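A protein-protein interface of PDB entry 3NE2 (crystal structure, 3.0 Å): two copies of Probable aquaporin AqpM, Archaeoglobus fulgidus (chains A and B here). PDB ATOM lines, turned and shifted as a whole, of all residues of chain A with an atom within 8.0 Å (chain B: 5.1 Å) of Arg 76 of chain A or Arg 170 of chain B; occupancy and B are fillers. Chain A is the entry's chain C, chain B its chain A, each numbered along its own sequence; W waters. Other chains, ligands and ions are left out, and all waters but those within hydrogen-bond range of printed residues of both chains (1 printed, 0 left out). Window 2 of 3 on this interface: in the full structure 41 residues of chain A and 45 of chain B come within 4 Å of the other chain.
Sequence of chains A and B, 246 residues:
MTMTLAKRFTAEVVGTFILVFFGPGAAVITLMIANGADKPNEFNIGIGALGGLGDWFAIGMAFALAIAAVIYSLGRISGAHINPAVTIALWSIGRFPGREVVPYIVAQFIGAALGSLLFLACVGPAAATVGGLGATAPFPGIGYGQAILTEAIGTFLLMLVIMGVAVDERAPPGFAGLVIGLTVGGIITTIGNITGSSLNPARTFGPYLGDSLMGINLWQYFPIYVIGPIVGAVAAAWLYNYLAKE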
ATOM      1  N   MET A   1     -17.646 -27.430   8.584  1.00  0.00           N
ATOM      2  CA  MET A   1     -18.936 -26.823   8.973  1.00  0.00           C
ATOM      3  C   MET A   1     -19.488 -27.407  10.275  1.00  0.00           C
ATOM      4  O   MET A   1     -20.708 -27.651  10.372  1.00  0.00           O
ATOM      5  CB  MET A   1     -19.986 -27.032   7.873  1.00  0.00           C
ATOM      6  CG  MET A   1     -19.928 -26.061   6.682  1.00  0.00           C
ATOM      7  SD  MET A   1     -21.402 -26.239   5.594  1.00  0.00           S
ATOM      8  CE  MET A   1     -22.758 -25.660   6.655  1.00  0.00           C
ATOM      9  N   THR A   2     -18.619 -27.666  11.259  1.00  0.00           N
ATOM     10  CA  THR A   2     -19.070 -27.716  12.679  1.00  0.00           C
ATOM     11  C   THR A   2     -18.958 -26.280  13.168  1.00  0.00           C
ATOM     12  O   THR A   2     -17.877 -25.751  13.462  1.00  0.00           O
ATOM     13  CB  THR A   2     -18.277 -28.692  13.611  1.00  0.00           C
ATOM     14  OG1 THR A   2     -18.327 -30.015  13.064  1.00  0.00           O
ATOM     15  CG2 THR A   2     -18.847 -28.697  15.083  1.00  0.00           C
ATOM     16  N   MET A   3     -20.110 -25.655  13.247  1.00  0.00           N
ATOM     17  CA  MET A   3     -20.174 -24.212  13.295  1.00  0.00           C
ATOM     18  C   MET A   3     -19.824 -23.681  14.689  1.00  0.00           C
ATOM     19  O   MET A   3     -20.057 -24.350  15.703  1.00  0.00           O
ATOM     20  CB  MET A   3     -21.575 -23.756  12.897  1.00  0.00           C
ATOM     21  CG  MET A   3     -21.980 -23.998  11.411  1.00  0.00           C
ATOM     22  SD  MET A   3     -20.976 -23.222  10.066  1.00  0.00           S
ATOM     23  CE  MET A   3     -20.223 -21.806  10.888  1.00  0.00           C
ATOM     24  N   ARG A   8     -24.117 -21.473  16.917  1.00  0.00           N
ATOM     25  CA  ARG A   8     -25.059 -22.486  17.438  1.00  0.00           C
ATOM     26  C   ARG A   8     -25.993 -21.867  18.495  1.00  0.00           C
ATOM     27  O   ARG A   8     -27.175 -22.262  18.624  1.00  0.00           O
ATOM     28  CB  ARG A   8     -24.317 -23.701  17.990  1.00  0.00           C
ATOM     29  CG  ARG A   8     -23.590 -24.452  16.890  1.00  0.00           C
ATOM     30  CD  ARG A   8     -22.807 -25.662  17.373  1.00  0.00           C
ATOM     31  NE  ARG A   8     -21.549 -25.300  18.020  1.00  0.00           N
ATOM     32  CZ  ARG A   8     -21.249 -25.532  19.294  1.00  0.00           C
ATOM     33  NH1 ARG A   8     -22.097 -26.133  20.124  1.00  0.00           N
ATOM     34  NH2 ARG A   8     -20.078 -25.152  19.742  1.00  0.00           N
ATOM     35  N   ALA A  11     -28.413 -19.977  16.467  1.00  0.00           N
ATOM     36  CA  ALA A  11     -29.257 -21.012  15.861  1.00  0.00           C
ATOM     37  C   ALA A  11     -30.292 -21.528  16.864  1.00  0.00           C
ATOM     38  O   ALA A  11     -31.461 -21.734  16.478  1.00  0.00           O
ATOM     39  CB  ALA A  11     -28.420 -22.146  15.323  1.00  0.00           C
ATOM     40  N   VAL A  70     -37.987 -26.837  12.059  1.00  0.00           N
ATOM     41  CA  VAL A  70     -36.753 -26.378  12.752  1.00  0.00           C
ATOM     42  C   VAL A  70     -35.574 -27.398  12.667  1.00  0.00           C
ATOM     43  O   VAL A  70     -34.454 -27.083  12.270  1.00  0.00           O
ATOM     44  CB  VAL A  70     -37.076 -25.990  14.268  1.00  0.00           C
ATOM     45  CG1 VAL A  70     -35.825 -25.879  15.112  1.00  0.00           C
ATOM     46  CG2 VAL A  70     -37.859 -24.686  14.344  1.00  0.00           C
ATOM     47  N   ILE A  71     -35.853 -28.625  13.055  1.00  0.00           N
ATOM     48  CA  ILE A  71     -34.865 -29.675  12.993  1.00  0.00           C
ATOM     49  C   ILE A  71     -34.338 -29.751  11.589  1.00  0.00           C
ATOM     50  O   ILE A  71     -33.146 -29.636  11.413  1.00  0.00           O
ATOM     51  CB  ILE A  71     -35.444 -31.059  13.416  1.00  0.00           C
ATOM     52  CG1 ILE A  71     -35.884 -31.067  14.901  1.00  0.00           C
ATOM     53  CG2 ILE A  71     -34.431 -32.124  13.179  1.00  0.00           C
ATOM     54  CD1 ILE A  71     -36.397 -32.419  15.368  1.00  0.00           C
ATOM     55  N   TYR A  72     -35.219 -29.911  10.603  1.00  0.00           N
ATOM     56  CA  TYR A  72     -34.803 -30.057   9.187  1.00  0.00           C
ATOM     57  C   TYR A  72     -34.032 -28.869   8.611  1.00  0.00           C
ATOM     58  O   TYR A  72     -33.303 -29.017   7.639  1.00  0.00           O
ATOM     59  CB  TYR A  72     -35.974 -30.335   8.251  1.00  0.00           C
ATOM     60  CG  TYR A  72     -36.463 -31.741   8.278  1.00  0.00           C
ATOM     61  CD1 TYR A  72     -35.654 -32.772   7.892  1.00  0.00           C
ATOM     62  CD2 TYR A  72     -37.765 -32.045   8.680  1.00  0.00           C
ATOM     63  CE1 TYR A  72     -36.099 -34.092   7.919  1.00  0.00           C
ATOM     64  CE2 TYR A  72     -38.224 -33.354   8.707  1.00  0.00           C
ATOM     65  CZ  TYR A  72     -37.378 -34.369   8.318  1.00  0.00           C
ATOM     66  OH  TYR A  72     -37.829 -35.654   8.336  1.00  0.00           O
ATOM     67  N   SER A  73     -34.208 -27.689   9.189  1.00  0.00           N
ATOM     68  CA  SER A  73     -33.491 -26.503   8.708  1.00  0.00           C
ATOM     69  C   SER A  73     -32.240 -26.165   9.539  1.00  0.00           C
ATOM     70  O   SER A  73     -31.212 -25.770   8.976  1.00  0.00           O
ATOM     71  CB  SER A  73     -34.457 -25.284   8.609  1.00  0.00           C
ATOM     72  OG  SER A  73     -35.241 -25.003   9.795  1.00  0.00           O
ATOM     73  N   LEU A  74     -32.335 -26.330  10.873  1.00  0.00           N
ATOM     74  CA  LEU A  74     -31.281 -25.893  11.806  1.00  0.00           C
ATOM     75  C   LEU A  74     -30.536 -26.987  12.597  1.00  0.00           C
ATOM     76  O   LEU A  74     -29.417 -26.732  13.106  1.00  0.00           O
ATOM     77  CB  LEU A  74     -31.878 -24.895  12.772  1.00  0.00           C
ATOM     78  CG  LEU A  74     -31.766 -23.470  12.280  1.00  0.00           C
ATOM     79  CD1 LEU A  74     -32.420 -23.297  10.975  1.00  0.00           C
ATOM     80  CD2 LEU A  74     -32.422 -22.585  13.307  1.00  0.00           C
ATOM     81  N   GLY A  75     -31.133 -28.189  12.673  1.00  0.00           N
ATOM     82  CA  GLY A  75     -30.509 -29.353  13.340  1.00  0.00           C
ATOM     83  C   GLY A  75     -29.040 -29.544  12.954  1.00  0.00           C
ATOM     84  O   GLY A  75     -28.158 -29.662  13.809  1.00  0.00           O
ATOM     85  N   ARG A  76     -28.777 -29.522  11.641  1.00  0.00           N
ATOM     86  CA  ARG A  76     -27.438 -29.584  11.125  1.00  0.00           C
ATOM     87  C   ARG A  76     -26.558 -28.511  11.712  1.00  0.00           C
ATOM     88  O   ARG A  76     -25.357 -28.639  11.628  1.00  0.00           O
ATOM     89  CB  ARG A  76     -27.437 -29.479   9.616  1.00  0.00           C
ATOM     90  CG  ARG A  76     -27.461 -30.851   8.925  1.00  0.00           C
ATOM     91  CD  ARG A  76     -26.866 -30.778   7.499  1.00  0.00           C
ATOM     92  NE  ARG A  76     -27.544 -29.709   6.794  1.00  0.00           N
ATOM     93  CZ  ARG A  76     -28.771 -29.812   6.292  1.00  0.00           C
ATOM     94  NH1 ARG A  76     -29.431 -30.962   6.353  1.00  0.00           N
ATOM     95  NH2 ARG A  76     -29.348 -28.768   5.706  1.00  0.00           N
ATOM     96  N   ILE A  77     -27.117 -27.460  12.315  1.00  0.00           N
ATOM     97  CA  ILE A  77     -26.281 -26.360  12.844  1.00  0.00           C
ATOM     98  C   ILE A  77     -26.028 -26.407  14.345  1.00  0.00           C
ATOM     99  O   ILE A  77     -24.894 -26.493  14.772  1.00  0.00           O
ATOM    100  CB  ILE A  77     -26.822 -24.961  12.445  1.00  0.00           C
ATOM    101  CG1 ILE A  77     -26.578 -24.745  10.943  1.00  0.00           C
ATOM    102  CG2 ILE A  77     -26.143 -23.837  13.285  1.00  0.00           C
ATOM    103  CD1 ILE A  77     -27.597 -23.843  10.307  1.00  0.00           C
ATOM    104  N   SER A  78     -27.082 -26.327  15.129  1.00  0.00           N
ATOM    105  CA  SER A  78     -26.972 -26.310  16.602  1.00  0.00           C
ATOM    106  C   SER A  78     -27.258 -27.674  17.213  1.00  0.00           C
ATOM    107  O   SER A  78     -27.019 -27.900  18.383  1.00  0.00           O
ATOM    108  CB  SER A  78     -27.993 -25.324  17.211  1.00  0.00           C
ATOM    109  OG  SER A  78     -29.384 -25.752  17.093  1.00  0.00           O
ATOM    110  N   GLY A  79     -27.834 -28.565  16.422  1.00  0.00           N
ATOM    111  CA  GLY A  79     -28.425 -29.775  16.959  1.00  0.00           C
ATOM    112  C   GLY A  79     -29.938 -29.631  17.067  1.00  0.00           C
ATOM    113  O   GLY A  79     -30.649 -30.640  17.226  1.00  0.00           O
ATOM    114  N   ALA A  80     -30.427 -28.387  16.960  1.00  0.00           N
ATOM    115  CA  ALA A  80     -31.840 -28.069  17.091  1.00  0.00           C
ATOM    116  C   ALA A  80     -32.426 -28.610  18.394  1.00  0.00           C
ATOM    117  O   ALA A  80     -33.450 -29.306  18.371  1.00  0.00           O
ATOM    118  CB  ALA A  80     -32.638 -28.596  15.902  1.00  0.00           C
ATOM    119  N   MET B 163     -34.565 -23.723   2.591  1.00  0.00           N
ATOM    120  CA  MET B 163     -33.095 -23.733   2.564  1.00  0.00           C
ATOM    121  C   MET B 163     -32.577 -25.042   3.102  1.00  0.00           C
ATOM    122  O   MET B 163     -31.688 -25.660   2.518  1.00  0.00           O
ATOM    123  CB  MET B 163     -32.537 -22.583   3.419  1.00  0.00           C
ATOM    124  CG  MET B 163     -32.872 -21.166   2.904  1.00  0.00           C
ATOM    125  SD  MET B 163     -32.207 -20.841   1.262  1.00  0.00           S
ATOM    126  CE  MET B 163     -30.467 -21.276   1.602  1.00  0.00           C
ATOM    127  N   GLY B 164     -33.173 -25.434   4.225  1.00  0.00           N
ATOM    128  CA  GLY B 164     -32.693 -26.519   5.046  1.00  0.00           C
ATOM    129  C   GLY B 164     -32.983 -27.902   4.534  1.00  0.00           C
ATOM    130  O   GLY B 164     -32.219 -28.830   4.825  1.00  0.00           O
ATOM    131  N   ASP B 168     -29.969 -26.857   0.505  1.00  0.00           N
ATOM    132  CA  ASP B 168     -28.728 -27.370   1.115  1.00  0.00           C
ATOM    133  C   ASP B 168     -28.334 -28.794   0.644  1.00  0.00           C
ATOM    134  O   ASP B 168     -29.030 -29.797   0.870  1.00  0.00           O
ATOM    135  CB  ASP B 168     -28.842 -27.354   2.633  1.00  0.00           C
ATOM    136  CG  ASP B 168     -27.499 -27.468   3.329  1.00  0.00           C
ATOM    137  OD1 ASP B 168     -27.295 -26.728   4.304  1.00  0.00           O
ATOM    138  OD2 ASP B 168     -26.650 -28.293   2.946  1.00  0.00           O
ATOM    139  N   GLU B 169     -27.166 -28.849   0.032  1.00  0.00           N
ATOM    140  CA  GLU B 169     -26.547 -30.085  -0.448  1.00  0.00           C
ATOM    141  C   GLU B 169     -26.594 -31.263   0.504  1.00  0.00           C
ATOM    142  O   GLU B 169     -26.597 -32.416   0.058  1.00  0.00           O
ATOM    143  CB  GLU B 169     -25.087 -29.782  -0.745  1.00  0.00           C
ATOM    144  CG  GLU B 169     -24.875 -28.374  -1.390  1.00  0.00           C
ATOM    145  CD  GLU B 169     -25.911 -28.044  -2.532  1.00  0.00           C
ATOM    146  OE1 GLU B 169     -27.075 -27.622  -2.186  1.00  0.00           O
ATOM    147  OE2 GLU B 169     -25.537 -28.219  -3.749  1.00  0.00           O
ATOM    148  N   ARG B 170     -26.613 -30.958   1.814  1.00  0.00           N
ATOM    149  CA  ARG B 170     -26.623 -31.974   2.882  1.00  0.00           C
ATOM    150  C   ARG B 170     -28.026 -32.408   3.285  1.00  0.00           C
ATOM    151  O   ARG B 170     -28.164 -33.198   4.204  1.00  0.00           O
ATOM    152  CB  ARG B 170     -25.807 -31.523   4.114  1.00  0.00           C
ATOM    153  CG  ARG B 170     -24.273 -31.808   3.987  1.00  0.00           C
ATOM    154  CD  ARG B 170     -23.598 -32.584   5.153  1.00  0.00           C
ATOM    155  NE  ARG B 170     -23.135 -31.672   6.207  1.00  0.00           N
ATOM    156  CZ  ARG B 170     -23.389 -31.779   7.529  1.00  0.00           C
ATOM    157  NH1 ARG B 170     -24.074 -32.816   8.039  1.00  0.00           N
ATOM    158  NH2 ARG B 170     -22.914 -30.849   8.375  1.00  0.00           N
ATOM    159  N   ALA B 171     -29.052 -31.954   2.567  1.00  0.00           N
ATOM    160  CA  ALA B 171     -30.440 -32.310   2.918  1.00  0.00           C
ATOM    161  C   ALA B 171     -30.829 -33.745   2.507  1.00  0.00           C
ATOM    162  O   ALA B 171     -30.570 -34.173   1.380  1.00  0.00           O
ATOM    163  CB  ALA B 171     -31.447 -31.298   2.320  1.00  0.00           C
ATOM    164  N   PRO B 172     -31.488 -34.478   3.424  1.00  0.00           N
ATOM    165  CA  PRO B 172     -31.859 -35.865   3.191  1.00  0.00           C
ATOM    166  C   PRO B 172     -32.848 -35.954   2.045  1.00  0.00           C
ATOM    167  O   PRO B 172     -33.920 -35.360   2.110  1.00  0.00           O
ATOM    168  CB  PRO B 172     -32.523 -36.277   4.498  1.00  0.00           C
ATOM    169  CG  PRO B 172     -33.067 -35.028   5.064  1.00  0.00           C
ATOM    170  CD  PRO B 172     -32.133 -33.932   4.639  1.00  0.00           C
ATOM    171  N   TYR B 240     -29.945 -18.003   6.804  1.00  0.00           N
ATOM    172  CA  TYR B 240     -29.527 -19.406   6.685  1.00  0.00           C
ATOM    173  C   TYR B 240     -28.067 -19.575   6.325  1.00  0.00           C
ATOM    174  O   TYR B 240     -27.336 -20.297   6.992  1.00  0.00           O
ATOM    175  CB  TYR B 240     -30.350 -20.128   5.618  1.00  0.00           C
ATOM    176  CG  TYR B 240     -30.094 -21.619   5.668  1.00  0.00           C
ATOM    177  CD1 TYR B 240     -29.104 -22.201   4.886  1.00  0.00           C
ATOM    178  CD2 TYR B 240     -30.823 -22.444   6.548  1.00  0.00           C
ATOM    179  CE1 TYR B 240     -28.841 -23.568   4.971  1.00  0.00           C
ATOM    180  CE2 TYR B 240     -30.577 -23.808   6.631  1.00  0.00           C
ATOM    181  CZ  TYR B 240     -29.575 -24.370   5.838  1.00  0.00           C
ATOM    182  OH  TYR B 240     -29.283 -25.715   5.898  1.00  0.00           O
HETATM  183  O   HOH W   1     -27.237 -27.075   7.205  1.00  0.00           O
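NH2 of Arg 76 of chain A sits at hydrogen-bond distance from O of Gly 164 of chain B (3.0 Å).
The side-chain carboxylate (OD1) of Asp 168 of chain B lies within salt-bridge range of the guanidinium group (NH2) of Arg 76 of chain A.
O of Arg 170 of chain B is in hydrogen-bond range of NH1 of Arg 76 of chain A (3.4 Å).
The guanidinium group (NH2) of Arg 76 of chain A sits at hydrogen-bond distance from the side-chain hydroxyl (OH) of Tyr 240 of chain B, at 3.1 Å.
O of Gly 164 of chain B sits close to O of Tyr 72 of chain A, at 3.0 Å.
N of Asp 168 of chain B is in hydrogen-bond range of O of Met 163 of chain B, 2.9 Å away.
OD2 of Asp 168 of chain B sits at hydrogen-bond distance from N of Arg 170 of chain B, 2.9 Å away.
OH of Tyr 240 of chain B lies within hydrogen-bond range of OD1 of Asp 168 of chain B, at 2.7 Å.
O of Val 70 of chain A is in hydrogen-bond range of OG of Ser 73 of chain A (3.3 Å).
Ser 73 of chain A touches Gly 164 of chain B.
O of Ser 73 of chain A touches CE2 of Tyr 240 of chain B (3.1 Å).
Arg 76 of chain A touches Ala 171 of chain B.
Of chain A, only Arg 76 (3.4 Å) comes within 4 Å of Arg 170 of chain B.
Ala 171 of chain B touches just one residue of chain A: Arg 76 (3.8 Å).
Of the printed residues of chain A, Gly 164 of chain B touches Tyr 72, Ser 73 and Arg 76.
Of the printed residues of chain A, Asp 168 of chain B touches Arg 76.
Printed residues of chain A within 4 Å of Tyr 240 of chain B: Ser 73 (3.1 Å) and Arg 76 (3.1 Å).
Of the printed residues of chain B, Tyr 72 of chain A touches Gly 164.
Gly 79 of chain A touches none of the printed residues of chain B.
The nearest residue of chain B that does not touch Arg 76 of chain A is Pro 172 of chain B (4.4 Å).
The nearest residue of chain A that does not touch Arg 170 of chain B is Met 1 of chain A (4.4 Å).
Of the 16 printed residues of chain A, 3 touch a printed residue of chain B.
Printed residues of chain B that touch a printed residue of chain A: Gly 164, Asp 168, Arg 170, Ala 171 and Tyr 240.
Hydrophobic or aromatic side chains of chain B within 4 Å of the printed part of chain A: Tyr 240.
Among the printed residues, Asp or Glu carboxylates within 4 Å of a Lys or Arg side-chain nitrogen of the other chain: Arg 76 of chain A with Asp 168 of chain B.
No position is printed for both chains.
Of the 8 pairs that touch across the chains among the printed residues, none has its exchanged pair printed and touching as well.
Water W1 lies within hydrogen-bond range of the guanidinium group of Arg 76 of chain A (2.7 Å), the side-chain hydroxyl of Tyr 240 of chain B (2.8 Å) and the side-chain carboxylate of Asp 168 of chain B (2.9 Å).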
